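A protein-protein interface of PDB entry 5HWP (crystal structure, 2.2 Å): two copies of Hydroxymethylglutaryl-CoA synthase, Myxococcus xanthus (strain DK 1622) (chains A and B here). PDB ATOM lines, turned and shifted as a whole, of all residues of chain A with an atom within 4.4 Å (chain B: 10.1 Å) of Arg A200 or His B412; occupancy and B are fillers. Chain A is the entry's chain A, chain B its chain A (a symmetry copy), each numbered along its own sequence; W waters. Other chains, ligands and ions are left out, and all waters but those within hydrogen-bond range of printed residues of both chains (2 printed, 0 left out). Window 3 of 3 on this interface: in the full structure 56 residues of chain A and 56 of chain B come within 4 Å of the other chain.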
ATOM      1  N   TRP A 195      21.946   6.657  14.998  1.00  0.00           N
ATOM      2  CA  TRP A 195      21.858   5.562  15.953  1.00  0.00           C
ATOM      3  C   TRP A 195      20.434   5.022  15.949  1.00  0.00           C
ATOM      4  O   TRP A 195      19.525   5.612  15.358  1.00  0.00           O
ATOM      5  CB  TRP A 195      22.302   6.009  17.356  1.00  0.00           C
ATOM      6  CG  TRP A 195      21.415   7.015  18.060  1.00  0.00           C
ATOM      7  CD1 TRP A 195      20.625   6.781  19.150  1.00  0.00           C
ATOM      8  CD2 TRP A 195      21.255   8.407  17.744  1.00  0.00           C
ATOM      9  NE1 TRP A 195      19.979   7.934  19.527  1.00  0.00           N
ATOM     10  CE2 TRP A 195      20.347   8.946  18.681  1.00  0.00           C
ATOM     11  CE3 TRP A 195      21.787   9.249  16.761  1.00  0.00           C
ATOM     12  CZ2 TRP A 195      19.958  10.286  18.660  1.00  0.00           C
ATOM     13  CZ3 TRP A 195      21.397  10.580  16.743  1.00  0.00           C
ATOM     14  CH2 TRP A 195      20.493  11.083  17.687  1.00  0.00           C
ATOM     15  N   ARG A 196      20.260   3.873  16.596  1.00  0.00           N
ATOM     16  CA  ARG A 196      18.966   3.190  16.643  1.00  0.00           C
ATOM     17  C   ARG A 196      18.869   2.461  17.976  1.00  0.00           C
ATOM     18  O   ARG A 196      19.364   1.331  18.116  1.00  0.00           O
ATOM     19  CB  ARG A 196      18.790   2.223  15.475  1.00  0.00           C
ATOM     20  CG  ARG A 196      17.397   1.610  15.401  1.00  0.00           C
ATOM     21  CD  ARG A 196      17.075   1.068  14.012  1.00  0.00           C
ATOM     22  NE  ARG A 196      17.793  -0.164  13.696  1.00  0.00           N
ATOM     23  CZ  ARG A 196      17.348  -1.389  13.966  1.00  0.00           C
ATOM     24  NH1 ARG A 196      16.180  -1.565  14.570  1.00  0.00           N
ATOM     25  NH2 ARG A 196      18.077  -2.447  13.632  1.00  0.00           N
ATOM     26  N   PRO A 197      18.250   3.073  18.986  1.00  0.00           N
ATOM     27  CA  PRO A 197      18.165   2.424  20.298  1.00  0.00           C
ATOM     28  C   PRO A 197      17.430   1.094  20.238  1.00  0.00           C
ATOM     29  O   PRO A 197      16.581   0.861  19.373  1.00  0.00           O
ATOM     30  CB  PRO A 197      17.403   3.446  21.150  1.00  0.00           C
ATOM     31  CG  PRO A 197      17.671   4.752  20.495  1.00  0.00           C
ATOM     32  CD  PRO A 197      17.751   4.460  19.027  1.00  0.00           C
ATOM     33  N   VAL A 198      17.768   0.215  21.185  1.00  0.00           N
ATOM     34  CA  VAL A 198      17.115  -1.084  21.272  1.00  0.00           C
ATOM     35  C   VAL A 198      15.612  -0.888  21.388  1.00  0.00           C
ATOM     36  O   VAL A 198      15.130  -0.032  22.143  1.00  0.00           O
ATOM     37  CB  VAL A 198      17.666  -1.881  22.466  1.00  0.00           C
ATOM     38  CG1 VAL A 198      16.955  -3.225  22.597  1.00  0.00           C
ATOM     39  CG2 VAL A 198      19.169  -2.085  22.321  1.00  0.00           C
ATOM     40  N   GLY A 199      14.859  -1.689  20.637  1.00  0.00           N
ATOM     41  CA  GLY A 199      13.419  -1.590  20.610  1.00  0.00           C
ATOM     42  C   GLY A 199      12.867  -0.676  19.538  1.00  0.00           C
ATOM     43  O   GLY A 199      11.711  -0.845  19.133  1.00  0.00           O
ATOM     44  N   ARG A 200      13.656   0.288  19.065  1.00  0.00           N
ATOM     45  CA  ARG A 200      13.220   1.187  18.008  1.00  0.00           C
ATOM     46  C   ARG A 200      13.526   0.567  16.652  1.00  0.00           C
ATOM     47  O   ARG A 200      14.663   0.165  16.385  1.00  0.00           O
ATOM     48  CB  ARG A 200      13.902   2.548  18.133  1.00  0.00           C
ATOM     49  CG  ARG A 200      13.264   3.616  17.264  1.00  0.00           C
ATOM     50  CD  ARG A 200      13.936   4.965  17.437  1.00  0.00           C
ATOM     51  NE  ARG A 200      13.243   6.011  16.686  1.00  0.00           N
ATOM     52  CZ  ARG A 200      12.333   6.839  17.195  1.00  0.00           C
ATOM     53  NH1 ARG A 200      11.766   7.751  16.414  1.00  0.00           N
ATOM     54  NH2 ARG A 200      11.990   6.773  18.476  1.00  0.00           N
ATOM     55  N   ARG A 201      12.506   0.493  15.802  1.00  0.00           N
ATOM     56  CA  ARG A 201      12.651  -0.125  14.492  1.00  0.00           C
ATOM     57  C   ARG A 201      13.193   0.842  13.448  1.00  0.00           C
ATOM     58  O   ARG A 201      13.773   0.394  12.452  1.00  0.00           O
ATOM     59  CB  ARG A 201      11.300  -0.672  14.039  1.00  0.00           C
ATOM     60  CG  ARG A 201      11.381  -1.913  13.181  1.00  0.00           C
ATOM     61  CD  ARG A 201      10.000  -2.503  12.994  1.00  0.00           C
ATOM     62  NE  ARG A 201       9.988  -3.605  12.038  1.00  0.00           N
ATOM     63  CZ  ARG A 201       8.882  -4.138  11.533  1.00  0.00           C
ATOM     64  NH1 ARG A 201       7.692  -3.669  11.888  1.00  0.00           N
ATOM     65  NH2 ARG A 201       8.964  -5.139  10.667  1.00  0.00           N
ATOM     66  N   GLU A 202      13.020   2.145  13.653  1.00  0.00           N
ATOM     67  CA  GLU A 202      13.512   3.165  12.740  1.00  0.00           C
ATOM     68  C   GLU A 202      14.709   3.875  13.356  1.00  0.00           C
ATOM     69  O   GLU A 202      14.746   4.119  14.566  1.00  0.00           O
ATOM     70  CB  GLU A 202      12.422   4.186  12.406  1.00  0.00           C
ATOM     71  CG  GLU A 202      11.431   3.716  11.351  1.00  0.00           C
ATOM     72  CD  GLU A 202      10.222   3.008  11.933  1.00  0.00           C
ATOM     73  OE1 GLU A 202      10.110   2.927  13.175  1.00  0.00           O
ATOM     74  OE2 GLU A 202       9.378   2.535  11.142  1.00  0.00           O
ATOM     75  N   LEU A 204      17.505   6.828  14.212  1.00  0.00           N
ATOM     76  CA  LEU A 204      17.584   8.251  14.504  1.00  0.00           C
ATOM     77  C   LEU A 204      18.828   8.810  13.831  1.00  0.00           C
ATOM     78  O   LEU A 204      19.874   8.156  13.806  1.00  0.00           O
ATOM     79  CB  LEU A 204      17.645   8.497  16.011  1.00  0.00           C
ATOM     80  CG  LEU A 204      16.456   7.947  16.800  1.00  0.00           C
ATOM     81  CD1 LEU A 204      16.783   7.883  18.281  1.00  0.00           C
ATOM     82  CD2 LEU A 204      15.226   8.803  16.554  1.00  0.00           C
ATOM     83  N   ILE B  88      23.315  -1.942  23.837  1.00  0.00           N
ATOM     84  CA  ILE B  88      22.375  -0.875  24.148  1.00  0.00           C
ATOM     85  C   ILE B  88      21.945  -0.113  22.900  1.00  0.00           C
ATOM     86  O   ILE B  88      21.211   0.868  23.001  1.00  0.00           O
ATOM     87  CB  ILE B  88      22.950   0.088  25.210  1.00  0.00           C
ATOM     88  CG1 ILE B  88      24.368   0.550  24.854  1.00  0.00           C
ATOM     89  CG2 ILE B  88      22.938  -0.574  26.575  1.00  0.00           C
ATOM     90  CD1 ILE B  88      24.447   1.609  23.769  1.00  0.00           C
ATOM     91  N   ASP B  89      22.380  -0.552  21.722  1.00  0.00           N
ATOM     92  CA  ASP B  89      21.968   0.074  20.474  1.00  0.00           C
ATOM     93  C   ASP B  89      22.165  -0.921  19.340  1.00  0.00           C
ATOM     94  O   ASP B  89      23.136  -1.681  19.341  1.00  0.00           O
ATOM     95  CB  ASP B  89      22.766   1.355  20.201  1.00  0.00           C
ATOM     96  CG  ASP B  89      22.087   2.260  19.194  1.00  0.00           C
ATOM     97  OD1 ASP B  89      21.254   3.095  19.611  1.00  0.00           O
ATOM     98  OD2 ASP B  89      22.385   2.141  17.988  1.00  0.00           O
ATOM     99  N   HIS B  90      21.239  -0.910  18.378  1.00  0.00           N
ATOM    100  CA  HIS B  90      21.389  -1.770  17.208  1.00  0.00           C
ATOM    101  C   HIS B  90      22.574  -1.345  16.350  1.00  0.00           C
ATOM    102  O   HIS B  90      23.153  -2.178  15.644  1.00  0.00           O
ATOM    103  CB  HIS B  90      20.115  -1.754  16.364  1.00  0.00           C
ATOM    104  CG  HIS B  90      18.955  -2.459  16.996  1.00  0.00           C
ATOM    105  ND1 HIS B  90      18.880  -3.831  17.089  1.00  0.00           N
ATOM    106  CD2 HIS B  90      17.816  -1.982  17.553  1.00  0.00           C
ATOM    107  CE1 HIS B  90      17.750  -4.170  17.683  1.00  0.00           C
ATOM    108  NE2 HIS B  90      17.086  -3.066  17.974  1.00  0.00           N
ATOM    109  N   SER B  91      22.945  -0.067  16.398  1.00  0.00           N
ATOM    110  CA  SER B  91      23.963   0.487  15.513  1.00  0.00           C
ATOM    111  C   SER B  91      25.190   0.986  16.256  1.00  0.00           C
ATOM    112  O   SER B  91      26.313   0.571  15.940  1.00  0.00           O
ATOM    113  CB  SER B  91      23.358   1.631  14.688  1.00  0.00           C
ATOM    114  OG  SER B  91      24.343   2.243  13.875  1.00  0.00           O
ATOM    115  N   LYS B  92      25.014   1.868  17.233  1.00  0.00           N
ATOM    116  CA  LYS B  92      26.150   2.483  17.909  1.00  0.00           C
ATOM    117  C   LYS B  92      26.750   1.499  18.908  1.00  0.00           C
ATOM    118  O   LYS B  92      26.039   1.041  19.810  1.00  0.00           O
ATOM    119  CB  LYS B  92      25.711   3.758  18.616  1.00  0.00           C
ATOM    120  CG  LYS B  92      26.838   4.536  19.274  1.00  0.00           C
ATOM    121  CD  LYS B  92      26.345   5.892  19.751  1.00  0.00           C
ATOM    122  CE  LYS B  92      27.400   6.621  20.572  1.00  0.00           C
ATOM    123  NZ  LYS B  92      28.603   6.969  19.769  1.00  0.00           N
ATOM    124  N   HIS B  97      30.975   4.429  22.819  1.00  0.00           N
ATOM    125  CA  HIS B  97      30.709   5.091  24.092  1.00  0.00           C
ATOM    126  C   HIS B  97      31.949   5.075  24.978  1.00  0.00           C
ATOM    127  O   HIS B  97      32.340   6.105  25.543  1.00  0.00           O
ATOM    128  CB  HIS B  97      29.538   4.414  24.808  1.00  0.00           C
ATOM    129  CG  HIS B  97      28.193   4.797  24.274  1.00  0.00           C
ATOM    130  ND1 HIS B  97      27.703   6.083  24.348  1.00  0.00           N
ATOM    131  CD2 HIS B  97      27.226   4.060  23.677  1.00  0.00           C
ATOM    132  CE1 HIS B  97      26.497   6.123  23.811  1.00  0.00           C
ATOM    133  NE2 HIS B  97      26.184   4.908  23.396  1.00  0.00           N
ATOM    134  N   VAL B 198      15.422  -9.571  20.715  1.00  0.00           N
ATOM    135  CA  VAL B 198      15.396  -8.118  20.826  1.00  0.00           C
ATOM    136  C   VAL B 198      14.117  -7.686  21.524  1.00  0.00           C
ATOM    137  O   VAL B 198      13.022  -8.187  21.229  1.00  0.00           O
ATOM    138  CB  VAL B 198      15.518  -7.473  19.436  1.00  0.00           C
ATOM    139  CG1 VAL B 198      15.445  -5.952  19.534  1.00  0.00           C
ATOM    140  CG2 VAL B 198      16.816  -7.901  18.762  1.00  0.00           C
ATOM    141  N   GLY B 199      14.249  -6.745  22.457  1.00  0.00           N
ATOM    142  CA  GLY B 199      13.129  -6.266  23.231  1.00  0.00           C
ATOM    143  C   GLY B 199      12.899  -7.004  24.532  1.00  0.00           C
ATOM    144  O   GLY B 199      12.295  -6.437  25.451  1.00  0.00           O
ATOM    145  N   ASP B 392      15.901   3.083  31.694  1.00  0.00           N
ATOM    146  CA  ASP B 392      16.191   4.508  31.610  1.00  0.00           C
ATOM    147  C   ASP B 392      15.966   5.233  32.934  1.00  0.00           C
ATOM    148  O   ASP B 392      15.772   6.453  32.937  1.00  0.00           O
ATOM    149  CB  ASP B 392      15.336   5.155  30.521  1.00  0.00           C
ATOM    150  CG  ASP B 392      13.873   5.244  30.907  1.00  0.00           C
ATOM    151  OD1 ASP B 392      13.424   4.424  31.736  1.00  0.00           O
ATOM    152  OD2 ASP B 392      13.174   6.134  30.381  1.00  0.00           O
ATOM    153  N   LEU B 406      25.450   5.537  34.078  1.00  0.00           N
ATOM    154  CA  LEU B 406      24.410   6.167  33.277  1.00  0.00           C
ATOM    155  C   LEU B 406      23.571   7.064  34.177  1.00  0.00           C
ATOM    156  O   LEU B 406      23.173   6.660  35.273  1.00  0.00           O
ATOM    157  CB  LEU B 406      23.536   5.105  32.610  1.00  0.00           C
ATOM    158  CG  LEU B 406      22.375   5.569  31.724  1.00  0.00           C
ATOM    159  CD1 LEU B 406      22.873   6.114  30.394  1.00  0.00           C
ATOM    160  CD2 LEU B 406      21.396   4.426  31.496  1.00  0.00           C
ATOM    161  N   GLU B 408      20.914   9.331  32.679  1.00  0.00           N
ATOM    162  CA  GLU B 408      19.603   9.555  32.088  1.00  0.00           C
ATOM    163  C   GLU B 408      19.709   9.300  30.591  1.00  0.00           C
ATOM    164  O   GLU B 408      20.806   9.212  30.031  1.00  0.00           O
ATOM    165  CB  GLU B 408      19.103  10.977  32.342  1.00  0.00           C
ATOM    166  CG  GLU B 408      20.090  12.047  31.894  1.00  0.00           C
ATOM    167  CD  GLU B 408      19.503  13.442  31.927  1.00  0.00           C
ATOM    168  OE1 GLU B 408      18.297  13.581  32.223  1.00  0.00           O
ATOM    169  OE2 GLU B 408      20.250  14.403  31.653  1.00  0.00           O
ATOM    170  N   ILE B 409      18.551   9.187  29.953  1.00  0.00           N
ATOM    171  CA  ILE B 409      18.439   9.121  28.502  1.00  0.00           C
ATOM    172  C   ILE B 409      17.556  10.289  28.083  1.00  0.00           C
ATOM    173  O   ILE B 409      16.353  10.303  28.375  1.00  0.00           O
ATOM    174  CB  ILE B 409      17.863   7.782  28.024  1.00  0.00           C
ATOM    175  CG1 ILE B 409      18.757   6.630  28.496  1.00  0.00           C
ATOM    176  CG2 ILE B 409      17.729   7.771  26.503  1.00  0.00           C
ATOM    177  CD1 ILE B 409      18.207   5.247  28.206  1.00  0.00           C
ATOM    178  N   ARG B 410      18.151  11.271  27.413  1.00  0.00           N
ATOM    179  CA  ARG B 410      17.445  12.470  26.979  1.00  0.00           C
ATOM    180  C   ARG B 410      17.438  12.526  25.461  1.00  0.00           C
ATOM    181  O   ARG B 410      18.499  12.477  24.829  1.00  0.00           O
ATOM    182  CB  ARG B 410      18.098  13.732  27.551  1.00  0.00           C
ATOM    183  N   ASP B 411      16.243  12.634  24.881  1.00  0.00           N
ATOM    184  CA  ASP B 411      16.086  12.679  23.429  1.00  0.00           C
ATOM    185  C   ASP B 411      16.812  11.508  22.772  1.00  0.00           C
ATOM    186  O   ASP B 411      17.501  11.662  21.763  1.00  0.00           O
ATOM    187  CB  ASP B 411      16.580  14.013  22.870  1.00  0.00           C
ATOM    188  CG  ASP B 411      15.967  15.206  23.582  1.00  0.00           C
ATOM    189  OD1 ASP B 411      14.801  15.105  24.021  1.00  0.00           O
ATOM    190  OD2 ASP B 411      16.652  16.244  23.705  1.00  0.00           O
ATOM    191  N   HIS B 412      16.666  10.325  23.368  1.00  0.00           N
ATOM    192  CA  HIS B 412      17.230   9.077  22.865  1.00  0.00           C
ATOM    193  C   HIS B 412      18.753   9.055  22.908  1.00  0.00           C
ATOM    194  O   HIS B 412      19.366   8.129  22.362  1.00  0.00           O
ATOM    195  CB  HIS B 412      16.748   8.794  21.439  1.00  0.00           C
ATOM    196  CG  HIS B 412      15.266   8.914  21.276  1.00  0.00           C
ATOM    197  ND1 HIS B 412      14.390   7.946  21.719  1.00  0.00           N
ATOM    198  CD2 HIS B 412      14.503   9.892  20.733  1.00  0.00           C
ATOM    199  CE1 HIS B 412      13.151   8.321  21.449  1.00  0.00           C
ATOM    200  NE2 HIS B 412      13.193   9.499  20.851  1.00  0.00           N
ATOM    201  N   ARG B 413      19.382  10.042  23.538  1.00  0.00           N
ATOM    202  CA  ARG B 413      20.825  10.053  23.745  1.00  0.00           C
ATOM    203  C   ARG B 413      21.126   9.656  25.183  1.00  0.00           C
ATOM    204  O   ARG B 413      20.514  10.183  26.119  1.00  0.00           O
ATOM    205  CB  ARG B 413      21.419  11.431  23.454  1.00  0.00           C
ATOM    206  CG  ARG B 413      21.332  11.878  22.006  1.00  0.00           C
ATOM    207  CD  ARG B 413      21.640  13.363  21.902  1.00  0.00           C
ATOM    208  NE  ARG B 413      21.776  13.819  20.521  1.00  0.00           N
ATOM    209  CZ  ARG B 413      20.754  14.091  19.715  1.00  0.00           C
ATOM    210  NH1 ARG B 413      19.507  13.945  20.139  1.00  0.00           N
ATOM    211  NH2 ARG B 413      20.983  14.503  18.475  1.00  0.00           N
ATOM    212  N   ARG B 414      22.068   8.736  25.356  1.00  0.00           N
ATOM    213  CA  ARG B 414      22.463   8.288  26.684  1.00  0.00           C
ATOM    214  C   ARG B 414      23.501   9.243  27.267  1.00  0.00           C
ATOM    215  O   ARG B 414      24.456   9.628  26.585  1.00  0.00           O
ATOM    216  CB  ARG B 414      23.019   6.867  26.612  1.00  0.00           C
ATOM    217  CG  ARG B 414      22.056   5.875  25.963  1.00  0.00           C
ATOM    218  CD  ARG B 414      22.713   4.535  25.674  1.00  0.00           C
ATOM    219  NE  ARG B 414      22.816   3.698  26.866  1.00  0.00           N
ATOM    220  CZ  ARG B 414      21.836   2.928  27.330  1.00  0.00           C
ATOM    221  NH1 ARG B 414      20.663   2.882  26.711  1.00  0.00           N
ATOM    222  NH2 ARG B 414      22.028   2.201  28.422  1.00  0.00           N
ATOM    223  N   GLN B 415      23.309   9.621  28.530  1.00  0.00           N
ATOM    224  CA  GLN B 415      24.195  10.543  29.226  1.00  0.00           C
ATOM    225  C   GLN B 415      24.871   9.814  30.376  1.00  0.00           C
ATOM    226  O   GLN B 415      24.231   9.033  31.088  1.00  0.00           O
ATOM    227  CB  GLN B 415      23.428  11.758  29.766  1.00  0.00           C
ATOM    228  CG  GLN B 415      22.434  12.370  28.786  1.00  0.00           C
ATOM    229  CD  GLN B 415      23.104  12.989  27.575  1.00  0.00           C
ATOM    230  OE1 GLN B 415      24.216  13.510  27.663  1.00  0.00           O
ATOM    231  NE2 GLN B 415      22.429  12.931  26.434  1.00  0.00           N
ATOM    232  N   TYR B 416      26.161  10.075  30.565  1.00  0.00           N
ATOM    233  CA  TYR B 416      26.945   9.399  31.584  1.00  0.00           C
ATOM    234  C   TYR B 416      27.691  10.415  32.435  1.00  0.00           C
ATOM    235  O   TYR B 416      27.939  11.549  32.017  1.00  0.00           O
ATOM    236  CB  TYR B 416      27.938   8.417  30.954  1.00  0.00           C
ATOM    237  CG  TYR B 416      27.258   7.279  30.235  1.00  0.00           C
ATOM    238  CD1 TYR B 416      26.819   7.426  28.926  1.00  0.00           C
ATOM    239  CD2 TYR B 416      27.042   6.064  30.867  1.00  0.00           C
ATOM    240  CE1 TYR B 416      26.190   6.392  28.267  1.00  0.00           C
ATOM    241  CE2 TYR B 416      26.413   5.025  30.217  1.00  0.00           C
ATOM    242  CZ  TYR B 416      25.989   5.193  28.917  1.00  0.00           C
ATOM    243  OH  TYR B 416      25.363   4.156  28.268  1.00  0.00           O
HETATM  244  O   HOH W   1      18.466   1.108  23.996  1.00  0.00           O
HETATM  245  O   HOH W   2       9.958   9.259  19.636  1.00  0.00           O
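NE1 of Trp A195 sits at hydrogen-bond distance from O of His B412, 2.9 Å away. The backbone NH (N) of Arg A196 lies within hydrogen-bond range of the side-chain carboxylate (OD2) of Asp B89, 3.1 Å away. N of His B90 lies within hydrogen-bond range of O of Arg A196. The side-chain carboxylate of Asp B89 sits close to the backbone nitrogen of Pro A197.
O of Trp A195 sits at hydrogen-bond distance from N of Leu A204. The backbone carbonyl oxygen of Arg A200 sits at hydrogen-bond distance from the guanidinium group of Arg A196 (2.9 Å). The guanidinium group (NE) of Arg A200 sits close to the backbone carbonyl oxygen (O) of Glu A202 (3.2 Å). The backbone NH (N) of Ser B91 lies within hydrogen-bond range of the side-chain carboxylate (OD2) of Asp B89 (2.8 Å). The backbone NH (N) of Lys B92 sits at hydrogen-bond distance from the side-chain carboxylate (OD2) of Asp B89. NH1 of Arg B413 is in hydrogen-bond range of O of Asp B411 (3.4 Å).
Trp A195 touches Asp B89. Trp A195 touches Arg B413. His B90 touches Pro A197 (CD2 to O, 3.6 Å). C of Ile B88 touches CG2 of Val A198, at 3.5 Å. N of Asp B89 touches CG2 of Val A198 (3.6 Å). His B90 touches Val A198 (NE2 to CA, 3.8 Å). Gly A199 touches His B90. CD2 of His B90 touches O of Arg A200, at 3.99 Å. Arg A200 touches His B412 (NH2 to CE1, 3.5 Å). CB of His B412 touches CD1 of Leu A204, 3.3 Å away.
Printed residues of chain B within 4 Å of Arg A196: Asp B89 (3.0 Å) and His B90 (2.9 Å). Printed residues of chain B within 4 Å of Val A198: Ile B88 (3.5 Å), Asp B89 (3.6 Å) and His B90 (3.8 Å). Printed residues of chain B within 4 Å of Arg A200: His B90 and His B412. Printed residues of chain B within 4 Å of Leu A204: His B412. Of the printed residues of chain A, His B90 touches Arg A196, Pro A197, Val A198, Gly A199 and Arg A200. Glu B408 touches none of the printed residues of chain A. His B412 touches three residues of chain A. Of the printed residues of chain A, Arg B413 touches Trp A195.
Hydrophobic or aromatic side chains of chain A within 4 Å of the printed part of chain B: Trp A195, Pro A197, Val A198 and Leu A204. Printed residues of chain B that touch a printed residue of chain A: Ile B88, Asp B89, His B90, His B412 and Arg B413. Among the printed residues, 14 pairs touch across the chains.
2 positions are printed for both chains. Of the 14 pairs that touch across the chains among the printed residues, none has its exchanged pair printed and touching as well.
Water W1 lies within hydrogen-bond range of O of Ile B88 (2.9 Å) and N of Val A198 (3.0 Å). Water W2 bridges the guanidinium group (NH2) of Arg A200 (3.4 Å) and a ring nitrogen (NE2) of His B412 (3.5 Å).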
